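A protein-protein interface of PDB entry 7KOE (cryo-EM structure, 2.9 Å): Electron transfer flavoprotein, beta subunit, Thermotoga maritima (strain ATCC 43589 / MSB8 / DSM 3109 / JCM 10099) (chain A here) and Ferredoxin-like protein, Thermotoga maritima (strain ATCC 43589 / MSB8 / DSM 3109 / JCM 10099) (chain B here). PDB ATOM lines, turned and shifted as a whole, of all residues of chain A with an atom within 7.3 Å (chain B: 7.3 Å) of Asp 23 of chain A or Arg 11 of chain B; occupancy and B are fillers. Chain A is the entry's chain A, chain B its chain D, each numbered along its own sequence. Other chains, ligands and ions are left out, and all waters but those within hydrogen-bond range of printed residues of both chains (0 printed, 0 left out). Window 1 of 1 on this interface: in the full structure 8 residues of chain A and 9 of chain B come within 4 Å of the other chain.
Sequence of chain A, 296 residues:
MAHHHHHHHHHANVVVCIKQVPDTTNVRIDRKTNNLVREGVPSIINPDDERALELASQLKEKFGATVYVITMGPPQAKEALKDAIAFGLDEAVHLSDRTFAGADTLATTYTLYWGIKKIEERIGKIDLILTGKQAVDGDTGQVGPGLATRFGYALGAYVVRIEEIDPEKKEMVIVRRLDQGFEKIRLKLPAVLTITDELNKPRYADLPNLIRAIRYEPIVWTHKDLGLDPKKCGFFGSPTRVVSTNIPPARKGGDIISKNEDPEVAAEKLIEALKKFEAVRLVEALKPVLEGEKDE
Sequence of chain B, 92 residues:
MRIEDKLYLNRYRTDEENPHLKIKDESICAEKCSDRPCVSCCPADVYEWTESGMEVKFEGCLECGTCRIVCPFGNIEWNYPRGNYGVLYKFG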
ATOM      1  N   VAL A  21      13.454  12.454  -3.277  1.00  0.00           N
ATOM      2  CA  VAL A  21      12.395  12.417  -4.278  1.00  0.00           C
ATOM      3  C   VAL A  21      12.778  13.424  -5.354  1.00  0.00           C
ATOM      4  O   VAL A  21      13.330  14.479  -5.020  1.00  0.00           O
ATOM      5  CB  VAL A  21      11.036  12.723  -3.622  1.00  0.00           C
ATOM      6  CG1 VAL A  21       9.945  12.993  -4.632  1.00  0.00           C
ATOM      7  CG2 VAL A  21      10.629  11.588  -2.715  1.00  0.00           C
ATOM      8  N   PRO A  22      12.574  13.132  -6.640  1.00  0.00           N
ATOM      9  CA  PRO A  22      12.784  14.156  -7.671  1.00  0.00           C
ATOM     10  C   PRO A  22      11.810  15.313  -7.512  1.00  0.00           C
ATOM     11  O   PRO A  22      10.713  15.159  -6.978  1.00  0.00           O
ATOM     12  CB  PRO A  22      12.537  13.399  -8.978  1.00  0.00           C
ATOM     13  CG  PRO A  22      12.751  11.977  -8.638  1.00  0.00           C
ATOM     14  CD  PRO A  22      12.315  11.808  -7.225  1.00  0.00           C
ATOM     15  N   ASP A  23      12.225  16.491  -7.972  1.00  0.00           N
ATOM     16  CA  ASP A  23      11.380  17.665  -7.813  1.00  0.00           C
ATOM     17  C   ASP A  23      10.220  17.601  -8.791  1.00  0.00           C
ATOM     18  O   ASP A  23      10.327  18.063  -9.931  1.00  0.00           O
ATOM     19  CB  ASP A  23      12.176  18.952  -8.009  1.00  0.00           C
ATOM     20  CG  ASP A  23      11.357  20.189  -7.707  1.00  0.00           C
ATOM     21  OD1 ASP A  23      11.331  20.621  -6.537  1.00  0.00           O
ATOM     22  OD2 ASP A  23      10.732  20.730  -8.639  1.00  0.00           O
ATOM     23  N   THR A  24       9.102  17.036  -8.339  1.00  0.00           N
ATOM     24  CA  THR A  24       7.970  16.733  -9.202  1.00  0.00           C
ATOM     25  C   THR A  24       7.161  17.955  -9.597  1.00  0.00           C
ATOM     26  O   THR A  24       6.261  17.828 -10.433  1.00  0.00           O
ATOM     27  CB  THR A  24       7.063  15.731  -8.512  1.00  0.00           C
ATOM     28  OG1 THR A  24       6.714  16.254  -7.228  1.00  0.00           O
ATOM     29  CG2 THR A  24       7.780  14.409  -8.351  1.00  0.00           C
ATOM     30  N   THR A  25       7.440  19.123  -9.019  1.00  0.00           N
ATOM     31  CA  THR A  25       6.916  20.354  -9.589  1.00  0.00           C
ATOM     32  C   THR A  25       7.526  20.633 -10.953  1.00  0.00           C
ATOM     33  O   THR A  25       6.900  21.305 -11.777  1.00  0.00           O
ATOM     34  CB  THR A  25       7.180  21.534  -8.655  1.00  0.00           C
ATOM     35  OG1 THR A  25       8.550  21.932  -8.766  1.00  0.00           O
ATOM     36  CG2 THR A  25       6.897  21.147  -7.222  1.00  0.00           C
ATOM     37  N   ASN A  26       8.727  20.117 -11.207  1.00  0.00           N
ATOM     38  CA  ASN A  26       9.394  20.259 -12.486  1.00  0.00           C
ATOM     39  C   ASN A  26       9.373  18.995 -13.332  1.00  0.00           C
ATOM     40  O   ASN A  26       9.562  19.085 -14.548  1.00  0.00           O
ATOM     41  CB  ASN A  26      10.848  20.689 -12.267  1.00  0.00           C
ATOM     42  CG  ASN A  26      11.465  21.274 -13.499  1.00  0.00           C
ATOM     43  OD1 ASN A  26      10.783  21.845 -14.344  1.00  0.00           O
ATOM     44  ND2 ASN A  26      12.767  21.125 -13.617  1.00  0.00           N
ATOM     45  N   VAL A  27       9.153  17.828 -12.731  1.00  0.00           N
ATOM     46  CA  VAL A  27       9.009  16.595 -13.498  1.00  0.00           C
ATOM     47  C   VAL A  27       7.674  16.664 -14.224  1.00  0.00           C
ATOM     48  O   VAL A  27       6.615  16.493 -13.616  1.00  0.00           O
ATOM     49  CB  VAL A  27       9.091  15.357 -12.605  1.00  0.00           C
ATOM     50  CG1 VAL A  27       8.903  14.107 -13.434  1.00  0.00           C
ATOM     51  CG2 VAL A  27      10.414  15.317 -11.874  1.00  0.00           C
ATOM     52  N   ARG A  28       7.717  16.929 -15.521  1.00  0.00           N
ATOM     53  CA  ARG A  28       6.521  17.224 -16.281  1.00  0.00           C
ATOM     54  C   ARG A  28       6.383  16.228 -17.420  1.00  0.00           C
ATOM     55  O   ARG A  28       7.300  15.465 -17.726  1.00  0.00           O
ATOM     56  CB  ARG A  28       6.553  18.656 -16.821  1.00  0.00           C
ATOM     57  CG  ARG A  28       7.447  18.810 -18.015  1.00  0.00           C
ATOM     58  CD  ARG A  28       7.883  20.232 -18.227  1.00  0.00           C
ATOM     59  NE  ARG A  28       8.840  20.325 -19.319  1.00  0.00           N
ATOM     60  CZ  ARG A  28      10.150  20.163 -19.172  1.00  0.00           C
ATOM     61  NH1 ARG A  28      10.656  19.902 -17.976  1.00  0.00           N
ATOM     62  NH2 ARG A  28      10.955  20.263 -20.219  1.00  0.00           N
ATOM     63  N   ARG A  38      12.298  13.991 -16.780  1.00  0.00           N
ATOM     64  CA  ARG A  38      12.822  14.137 -15.435  1.00  0.00           C
ATOM     65  C   ARG A  38      14.342  14.147 -15.399  1.00  0.00           C
ATOM     66  O   ARG A  38      14.922  14.100 -14.312  1.00  0.00           O
ATOM     67  CB  ARG A  38      12.290  13.016 -14.545  1.00  0.00           C
ATOM     68  CG  ARG A  38      12.266  11.664 -15.214  1.00  0.00           C
ATOM     69  CD  ARG A  38      11.817  10.585 -14.250  1.00  0.00           C
ATOM     70  NE  ARG A  38      12.610  10.594 -13.026  1.00  0.00           N
ATOM     71  CZ  ARG A  38      12.719   9.562 -12.197  1.00  0.00           C
ATOM     72  NH1 ARG A  38      12.088   8.427 -12.461  1.00  0.00           N
ATOM     73  NH2 ARG A  38      13.461   9.665 -11.104  1.00  0.00           N
ATOM     74  N   GLY A  40      17.936  15.908 -15.551  1.00  0.00           N
ATOM     75  CA  GLY A  40      18.389  17.208 -15.116  1.00  0.00           C
ATOM     76  C   GLY A  40      17.694  17.753 -13.893  1.00  0.00           C
ATOM     77  O   GLY A  40      18.264  18.610 -13.209  1.00  0.00           O
ATOM     78  N   VAL A  41      16.484  17.290 -13.594  1.00  0.00           N
ATOM     79  CA  VAL A  41      15.707  17.746 -12.446  1.00  0.00           C
ATOM     80  C   VAL A  41      16.357  17.211 -11.178  1.00  0.00           C
ATOM     81  O   VAL A  41      16.471  15.990 -11.013  1.00  0.00           O
ATOM     82  CB  VAL A  41      14.242  17.298 -12.550  1.00  0.00           C
ATOM     83  CG1 VAL A  41      13.457  17.799 -11.363  1.00  0.00           C
ATOM     84  CG2 VAL A  41      13.633  17.804 -13.835  1.00  0.00           C
ATOM     85  N   PRO A  42      16.804  18.076 -10.274  1.00  0.00           N
ATOM     86  CA  PRO A  42      17.506  17.596  -9.084  1.00  0.00           C
ATOM     87  C   PRO A  42      16.548  16.975  -8.088  1.00  0.00           C
ATOM     88  O   PRO A  42      15.352  17.267  -8.070  1.00  0.00           O
ATOM     89  CB  PRO A  42      18.151  18.865  -8.516  1.00  0.00           C
ATOM     90  CG  PRO A  42      18.068  19.869  -9.615  1.00  0.00           C
ATOM     91  CD  PRO A  42      16.821  19.540 -10.347  1.00  0.00           C
ATOM     92  N   SER A  43      17.092  16.101  -7.256  1.00  0.00           N
ATOM     93  CA  SER A  43      16.298  15.379  -6.282  1.00  0.00           C
ATOM     94  C   SER A  43      16.358  16.076  -4.933  1.00  0.00           C
ATOM     95  O   SER A  43      17.419  16.528  -4.498  1.00  0.00           O
ATOM     96  CB  SER A  43      16.786  13.939  -6.165  1.00  0.00           C
ATOM     97  OG  SER A  43      16.854  13.322  -7.437  1.00  0.00           O
ATOM     98  N   ILE A  44      15.208  16.151  -4.273  1.00  0.00           N
ATOM     99  CA  ILE A  44      15.064  16.914  -3.043  1.00  0.00           C
ATOM    100  C   ILE A  44      14.611  15.988  -1.931  1.00  0.00           C
ATOM    101  O   ILE A  44      14.480  14.779  -2.134  1.00  0.00           O
ATOM    102  CB  ILE A  44      14.062  18.063  -3.230  1.00  0.00           C
ATOM    103  CG1 ILE A  44      12.840  17.562  -3.992  1.00  0.00           C
ATOM    104  CG2 ILE A  44      14.701  19.186  -3.986  1.00  0.00           C
ATOM    105  CD1 ILE A  44      11.664  18.491  -3.950  1.00  0.00           C
ATOM    106  N   ILE A  45      14.387  16.544  -0.741  1.00  0.00           N
ATOM    107  CA  ILE A  45      13.603  15.838   0.259  1.00  0.00           C
ATOM    108  C   ILE A  45      12.178  15.717  -0.261  1.00  0.00           C
ATOM    109  O   ILE A  45      11.698  16.562  -1.028  1.00  0.00           O
ATOM    110  CB  ILE A  45      13.622  16.568   1.615  1.00  0.00           C
ATOM    111  CG1 ILE A  45      14.985  17.191   1.885  1.00  0.00           C
ATOM    112  CG2 ILE A  45      13.248  15.628   2.758  1.00  0.00           C
ATOM    113  CD1 ILE A  45      16.027  16.208   2.214  1.00  0.00           C
ATOM    114  N   PRO A  47       8.533  16.474   0.149  1.00  0.00           N
ATOM    115  CA  PRO A  47       7.949  17.616   0.869  1.00  0.00           C
ATOM    116  C   PRO A  47       7.049  17.231   2.027  1.00  0.00           C
ATOM    117  O   PRO A  47       6.829  18.064   2.912  1.00  0.00           O
ATOM    118  CB  PRO A  47       7.161  18.349  -0.222  1.00  0.00           C
ATOM    119  CG  PRO A  47       7.798  17.930  -1.487  1.00  0.00           C
ATOM    120  CD  PRO A  47       8.220  16.516  -1.285  1.00  0.00           C
ATOM    121  N   VAL A 136       6.546  11.263  -3.485  1.00  0.00           N
ATOM    122  CA  VAL A 136       5.839  11.729  -4.668  1.00  0.00           C
ATOM    123  C   VAL A 136       6.140  10.848  -5.876  1.00  0.00           C
ATOM    124  O   VAL A 136       5.271  10.677  -6.740  1.00  0.00           O
ATOM    125  CB  VAL A 136       6.151  13.205  -4.962  1.00  0.00           C
ATOM    126  CG1 VAL A 136       5.107  13.774  -5.899  1.00  0.00           C
ATOM    127  CG2 VAL A 136       6.190  14.004  -3.690  1.00  0.00           C
ATOM    128  N   LEU B   7       8.113  29.254 -19.346  1.00  0.00           N
ATOM    129  CA  LEU B   7       8.506  29.357 -17.948  1.00  0.00           C
ATOM    130  C   LEU B   7       8.145  28.111 -17.165  1.00  0.00           C
ATOM    131  O   LEU B   7       8.682  27.903 -16.075  1.00  0.00           O
ATOM    132  CB  LEU B   7       7.852  30.568 -17.291  1.00  0.00           C
ATOM    133  CG  LEU B   7       8.312  31.948 -17.739  1.00  0.00           C
ATOM    134  CD1 LEU B   7       7.711  32.977 -16.826  1.00  0.00           C
ATOM    135  CD2 LEU B   7       9.814  32.040 -17.736  1.00  0.00           C
ATOM    136  N   TYR B   8       7.237  27.290 -17.689  1.00  0.00           N
ATOM    137  CA  TYR B   8       6.935  26.011 -17.071  1.00  0.00           C
ATOM    138  C   TYR B   8       8.090  25.031 -17.209  1.00  0.00           C
ATOM    139  O   TYR B   8       8.205  24.106 -16.400  1.00  0.00           O
ATOM    140  CB  TYR B   8       5.660  25.433 -17.687  1.00  0.00           C
ATOM    141  CG  TYR B   8       5.203  24.149 -17.047  1.00  0.00           C
ATOM    142  CD1 TYR B   8       4.807  24.117 -15.720  1.00  0.00           C
ATOM    143  CD2 TYR B   8       5.189  22.965 -17.766  1.00  0.00           C
ATOM    144  CE1 TYR B   8       4.401  22.945 -15.131  1.00  0.00           C
ATOM    145  CE2 TYR B   8       4.782  21.789 -17.185  1.00  0.00           C
ATOM    146  CZ  TYR B   8       4.394  21.785 -15.866  1.00  0.00           C
ATOM    147  OH  TYR B   8       3.991  20.612 -15.281  1.00  0.00           O
ATOM    148  N   LEU B   9       8.954  25.228 -18.204  1.00  0.00           N
ATOM    149  CA  LEU B   9      10.107  24.359 -18.390  1.00  0.00           C
ATOM    150  C   LEU B   9      11.159  24.584 -17.319  1.00  0.00           C
ATOM    151  O   LEU B   9      11.881  23.650 -16.958  1.00  0.00           O
ATOM    152  CB  LEU B   9      10.711  24.605 -19.765  1.00  0.00           C
ATOM    153  CG  LEU B   9       9.708  24.571 -20.909  1.00  0.00           C
ATOM    154  CD1 LEU B   9      10.341  25.118 -22.149  1.00  0.00           C
ATOM    155  CD2 LEU B   9       9.211  23.170 -21.143  1.00  0.00           C
ATOM    156  N   ASN B  10      11.271  25.808 -16.815  1.00  0.00           N
ATOM    157  CA  ASN B  10      12.249  26.120 -15.790  1.00  0.00           C
ATOM    158  C   ASN B  10      11.842  25.504 -14.462  1.00  0.00           C
ATOM    159  O   ASN B  10      10.685  25.161 -14.231  1.00  0.00           O
ATOM    160  CB  ASN B  10      12.392  27.625 -15.609  1.00  0.00           C
ATOM    161  CG  ASN B  10      12.909  28.313 -16.828  1.00  0.00           C
ATOM    162  OD1 ASN B  10      12.274  29.212 -17.360  1.00  0.00           O
ATOM    163  ND2 ASN B  10      14.078  27.913 -17.271  1.00  0.00           N
ATOM    164  N   ARG B  11      12.816  25.375 -13.578  1.00  0.00           N
ATOM    165  CA  ARG B  11      12.575  24.885 -12.235  1.00  0.00           C
ATOM    166  C   ARG B  11      12.614  26.051 -11.269  1.00  0.00           C
ATOM    167  O   ARG B  11      13.536  26.866 -11.310  1.00  0.00           O
ATOM    168  CB  ARG B  11      13.610  23.842 -11.838  1.00  0.00           C
ATOM    169  CG  ARG B  11      13.247  23.106 -10.592  1.00  0.00           C
ATOM    170  CD  ARG B  11      14.463  22.512  -9.977  1.00  0.00           C
ATOM    171  NE  ARG B  11      14.182  21.990  -8.655  1.00  0.00           N
ATOM    172  CZ  ARG B  11      15.097  21.867  -7.709  1.00  0.00           C
ATOM    173  NH1 ARG B  11      16.343  22.232  -7.943  1.00  0.00           N
ATOM    174  NH2 ARG B  11      14.764  21.380  -6.533  1.00  0.00           N
ATOM    175  N   TYR B  12      11.615  26.128 -10.406  1.00  0.00           N
ATOM    176  CA  TYR B  12      11.521  27.194  -9.432  1.00  0.00           C
ATOM    177  C   TYR B  12      11.350  26.605  -8.047  1.00  0.00           C
ATOM    178  O   TYR B  12      10.761  25.540  -7.870  1.00  0.00           O
ATOM    179  CB  TYR B  12      10.342  28.118  -9.707  1.00  0.00           C
ATOM    180  CG  TYR B  12      10.426  28.933 -10.965  1.00  0.00           C
ATOM    181  CD1 TYR B  12      10.076  28.396 -12.191  1.00  0.00           C
ATOM    182  CD2 TYR B  12      10.821  30.250 -10.924  1.00  0.00           C
ATOM    183  CE1 TYR B  12      10.130  29.146 -13.331  1.00  0.00           C
ATOM    184  CE2 TYR B  12      10.875  31.002 -12.061  1.00  0.00           C
ATOM    185  CZ  TYR B  12      10.543  30.443 -13.260  1.00  0.00           C
ATOM    186  OH  TYR B  12      10.603  31.203 -14.396  1.00  0.00           O
ATOM    187  N   ARG B  13      11.872  27.314  -7.061  1.00  0.00           N
ATOM    188  CA  ARG B  13      11.384  27.204  -5.696  1.00  0.00           C
ATOM    189  C   ARG B  13      10.823  28.579  -5.377  1.00  0.00           C
ATOM    190  O   ARG B  13      11.573  29.515  -5.103  1.00  0.00           O
ATOM    191  CB  ARG B  13      12.460  26.782  -4.711  1.00  0.00           C
ATOM    192  CG  ARG B  13      11.866  26.424  -3.373  1.00  0.00           C
ATOM    193  CD  ARG B  13      12.815  25.679  -2.476  1.00  0.00           C
ATOM    194  NE  ARG B  13      13.034  24.304  -2.887  1.00  0.00           N
ATOM    195  CZ  ARG B  13      14.139  23.877  -3.478  1.00  0.00           C
ATOM    196  NH1 ARG B  13      15.114  24.724  -3.736  1.00  0.00           N
ATOM    197  NH2 ARG B  13      14.264  22.606  -3.812  1.00  0.00           N
ATOM    198  N   THR B  14       9.509  28.710  -5.453  1.00  0.00           N
ATOM    199  CA  THR B  14       8.877  30.003  -5.294  1.00  0.00           C
ATOM    200  C   THR B  14       8.777  30.369  -3.821  1.00  0.00           C
ATOM    201  O   THR B  14       8.458  29.529  -2.977  1.00  0.00           O
ATOM    202  CB  THR B  14       7.494  29.992  -5.933  1.00  0.00           C
ATOM    203  OG1 THR B  14       7.558  29.312  -7.189  1.00  0.00           O
ATOM    204  CG2 THR B  14       7.018  31.395  -6.174  1.00  0.00           C
ATOM    205  N   ASN B  84      18.239  29.392  -1.923  1.00  0.00           N
ATOM    206  CA  ASN B  84      17.412  28.243  -2.305  1.00  0.00           C
ATOM    207  C   ASN B  84      16.021  28.668  -2.762  1.00  0.00           C
ATOM    208  O   ASN B  84      15.046  27.967  -2.529  1.00  0.00           O
ATOM    209  CB  ASN B  84      17.311  27.207  -1.179  1.00  0.00           C
ATOM    210  CG  ASN B  84      17.302  25.801  -1.685  1.00  0.00           C
ATOM    211  OD1 ASN B  84      17.173  25.564  -2.879  1.00  0.00           O
ATOM    212  ND2 ASN B  84      17.429  24.847  -0.777  1.00  0.00           N
ATOM    213  N   GLY B  86      13.710  31.062  -6.017  1.00  0.00           N
ATOM    214  CA  GLY B  86      13.730  31.683  -7.326  1.00  0.00           C
ATOM    215  C   GLY B  86      13.935  30.676  -8.433  1.00  0.00           C
ATOM    216  O   GLY B  86      13.532  29.527  -8.270  1.00  0.00           O
ATOM    217  N   VAL B  87      14.533  31.079  -9.559  1.00  0.00           N
ATOM    218  CA  VAL B  87      14.906  30.119 -10.593  1.00  0.00           C
ATOM    219  C   VAL B  87      15.962  29.175 -10.058  1.00  0.00           C
ATOM    220  O   VAL B  87      16.832  29.558  -9.268  1.00  0.00           O
ATOM    221  CB  VAL B  87      15.424  30.799 -11.870  1.00  0.00           C
ATOM    222  CG1 VAL B  87      14.322  31.383 -12.639  1.00  0.00           C
ATOM    223  CG2 VAL B  87      16.422  31.874 -11.533  1.00  0.00           C
ATOM    224  N   LEU B  88      15.872  27.919 -10.465  1.00  0.00           N
ATOM    225  CA  LEU B  88      16.904  26.937 -10.184  1.00  0.00           C
ATOM    226  C   LEU B  88      17.230  26.327 -11.532  1.00  0.00           C
ATOM    227  O   LEU B  88      16.588  25.368 -11.957  1.00  0.00           O
ATOM    228  CB  LEU B  88      16.456  25.908  -9.166  1.00  0.00           C
ATOM    229  CG  LEU B  88      16.017  26.483  -7.822  1.00  0.00           C
ATOM    230  CD1 LEU B  88      15.275  25.448  -7.038  1.00  0.00           C
ATOM    231  CD2 LEU B  88      17.201  26.995  -7.045  1.00  0.00           C
ATOM    232  N   TYR B  89      18.213  26.908 -12.208  1.00  0.00           N
ATOM    233  CA  TYR B  89      18.543  26.491 -13.559  1.00  0.00           C
ATOM    234  C   TYR B  89      19.202  25.123 -13.540  1.00  0.00           C
ATOM    235  O   TYR B  89      20.275  24.947 -12.959  1.00  0.00           O
ATOM    236  CB  TYR B  89      19.466  27.502 -14.226  1.00  0.00           C
ATOM    237  CG  TYR B  89      18.825  28.810 -14.608  1.00  0.00           C
ATOM    238  CD1 TYR B  89      17.667  28.850 -15.363  1.00  0.00           C
ATOM    239  CD2 TYR B  89      19.395  30.006 -14.225  1.00  0.00           C
ATOM    240  CE1 TYR B  89      17.100  30.045 -15.720  1.00  0.00           C
ATOM    241  CE2 TYR B  89      18.834  31.198 -14.569  1.00  0.00           C
ATOM    242  CZ  TYR B  89      17.693  31.216 -15.318  1.00  0.00           C
ATOM    243  OH  TYR B  89      17.148  32.424 -15.658  1.00  0.00           O
ATOM    244  N   LYS B  90      18.541  24.151 -14.146  1.00  0.00           N
ATOM    245  CA  LYS B  90      19.155  22.871 -14.445  1.00  0.00           C
ATOM    246  C   LYS B  90      19.747  22.972 -15.845  1.00  0.00           C
ATOM    247  O   LYS B  90      19.097  23.499 -16.749  1.00  0.00           O
ATOM    248  CB  LYS B  90      18.124  21.745 -14.320  1.00  0.00           C
ATOM    249  CG  LYS B  90      16.903  21.878 -15.217  1.00  0.00           C
ATOM    250  CD  LYS B  90      15.878  20.810 -15.027  1.00  0.00           C
ATOM    251  CE  LYS B  90      14.879  20.904 -16.160  1.00  0.00           C
ATOM    252  NZ  LYS B  90      14.146  22.192 -16.146  1.00  0.00           N
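Of the 14 printed residues of chain B, 6 touch a printed residue of chain A. Printed residues of chain B that touch a printed residue of chain A: Tyr 8, Leu 9, Asn 10, Arg 11, Arg 13 and Lys 90. Hydrophobic or aromatic side chains of chain B that line the printed part of chain A: Tyr 8 and Leu 9. Among the printed residues, Asp or Glu carboxylates within 4 Å of a Lys or Arg side-chain nitrogen of the other chain: Asp 23 of chain A with Arg 11 of chain B (3.5 Å).
The backbone carbonyl oxygen (O) of Val 21 of chain A lies within hydrogen-bond range of the backbone NH (N) of Ile 44 of chain A, 2.6 Å away. OD2 of Asp 23 of chain A is in hydrogen-bond range of N of Asn 26 of chain A, 3.3 Å away. O of Pro 42 of chain A sits at hydrogen-bond distance from N of Asp 23 of chain A, at 3.2 Å. The backbone NH (N) of Leu 88 of chain B is in hydrogen-bond range of the backbone carbonyl oxygen (O) of Arg 11 of chain B (2.7 Å). The guanidinium group (NH1) of Arg 13 of chain B sits close to the backbone carbonyl oxygen (O) of Asn 84 of chain B (3.5 Å). The backbone carbonyl oxygen of Arg 13 of chain B is in hydrogen-bond range of the backbone NH of Gly 86 of chain B (2.8 Å).
Of chain B, only Arg 11 (3.5 Å) comes within 4 Å of Asp 23 of chain A. Of the printed residues of chain B, Asn 26 of chain A touches Tyr 8 (3.998 Å), Leu 9 (3.4 Å), Asn 10 (3.3 Å), Arg 11 (3.4 Å) and Lys 90 (3.1 Å). Printed residues of chain B within 4 Å of Gly 40 of chain A: Lys 90 (3.3 Å). Of the printed residues of chain B, Pro 42 of chain A touches Arg 11 (3.4 Å). Of the printed residues of chain A, Asn 10 of chain B touches Asn 26 (3.3 Å). Of chain A, only Asp 23 (3.5 Å), Asn 26 (3.4 Å), Pro 42 (3.4 Å) and Ile 44 (3.4 Å) come within 4 Å of Arg 11 of chain B. The nearest residue of chain B that does not touch Asp 23 of chain A is Arg 13 of chain B (4.5 Å). The nearest residue of chain A that does not touch Arg 11 of chain B is Val 41 of chain A (5.0 Å). The nearest printed residue of chain B that does not touch Asn 26 of chain A is Tyr 12 of chain B (5.8 Å).
NH2 of Arg 11 of chain B lies within salt-bridge range of OD1 of Asp 23 of chain A (3.5 Å). The side-chain amide oxygen of Asn 26 of chain A lies close to the backbone carbonyl oxygen of Leu 9 of chain B (3.4 Å). OD1 of Asn 26 of chain A lies close to O of Asn 10 of chain B (3.3 Å). The side-chain amide nitrogen (ND2) of Asn 26 of chain A sits close to the side-chain amino group (NZ) of Lys 90 of chain B.
Among the printed residues, merely in contact across the chains: Asn 26 of chain A with Tyr 8 of chain B (3.998 Å), Asn 26 of chain A with Arg 11 of chain B (3.4 Å), Arg 28 of chain A with Tyr 8 of chain B (3.6 Å), Arg 28 of chain A with Leu 9 of chain B (3.4 Å), Gly 40 of chain A with Lys 90 of chain B (3.3 Å), Val 41 of chain A with Lys 90 of chain B (3.8 Å), Pro 42 of chain A with Arg 11 of chain B (3.4 Å), Ile 44 of chain A with Arg 11 of chain B (3.4 Å) and Ile 44 of chain A with Arg 13 of chain B (3.5 Å).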
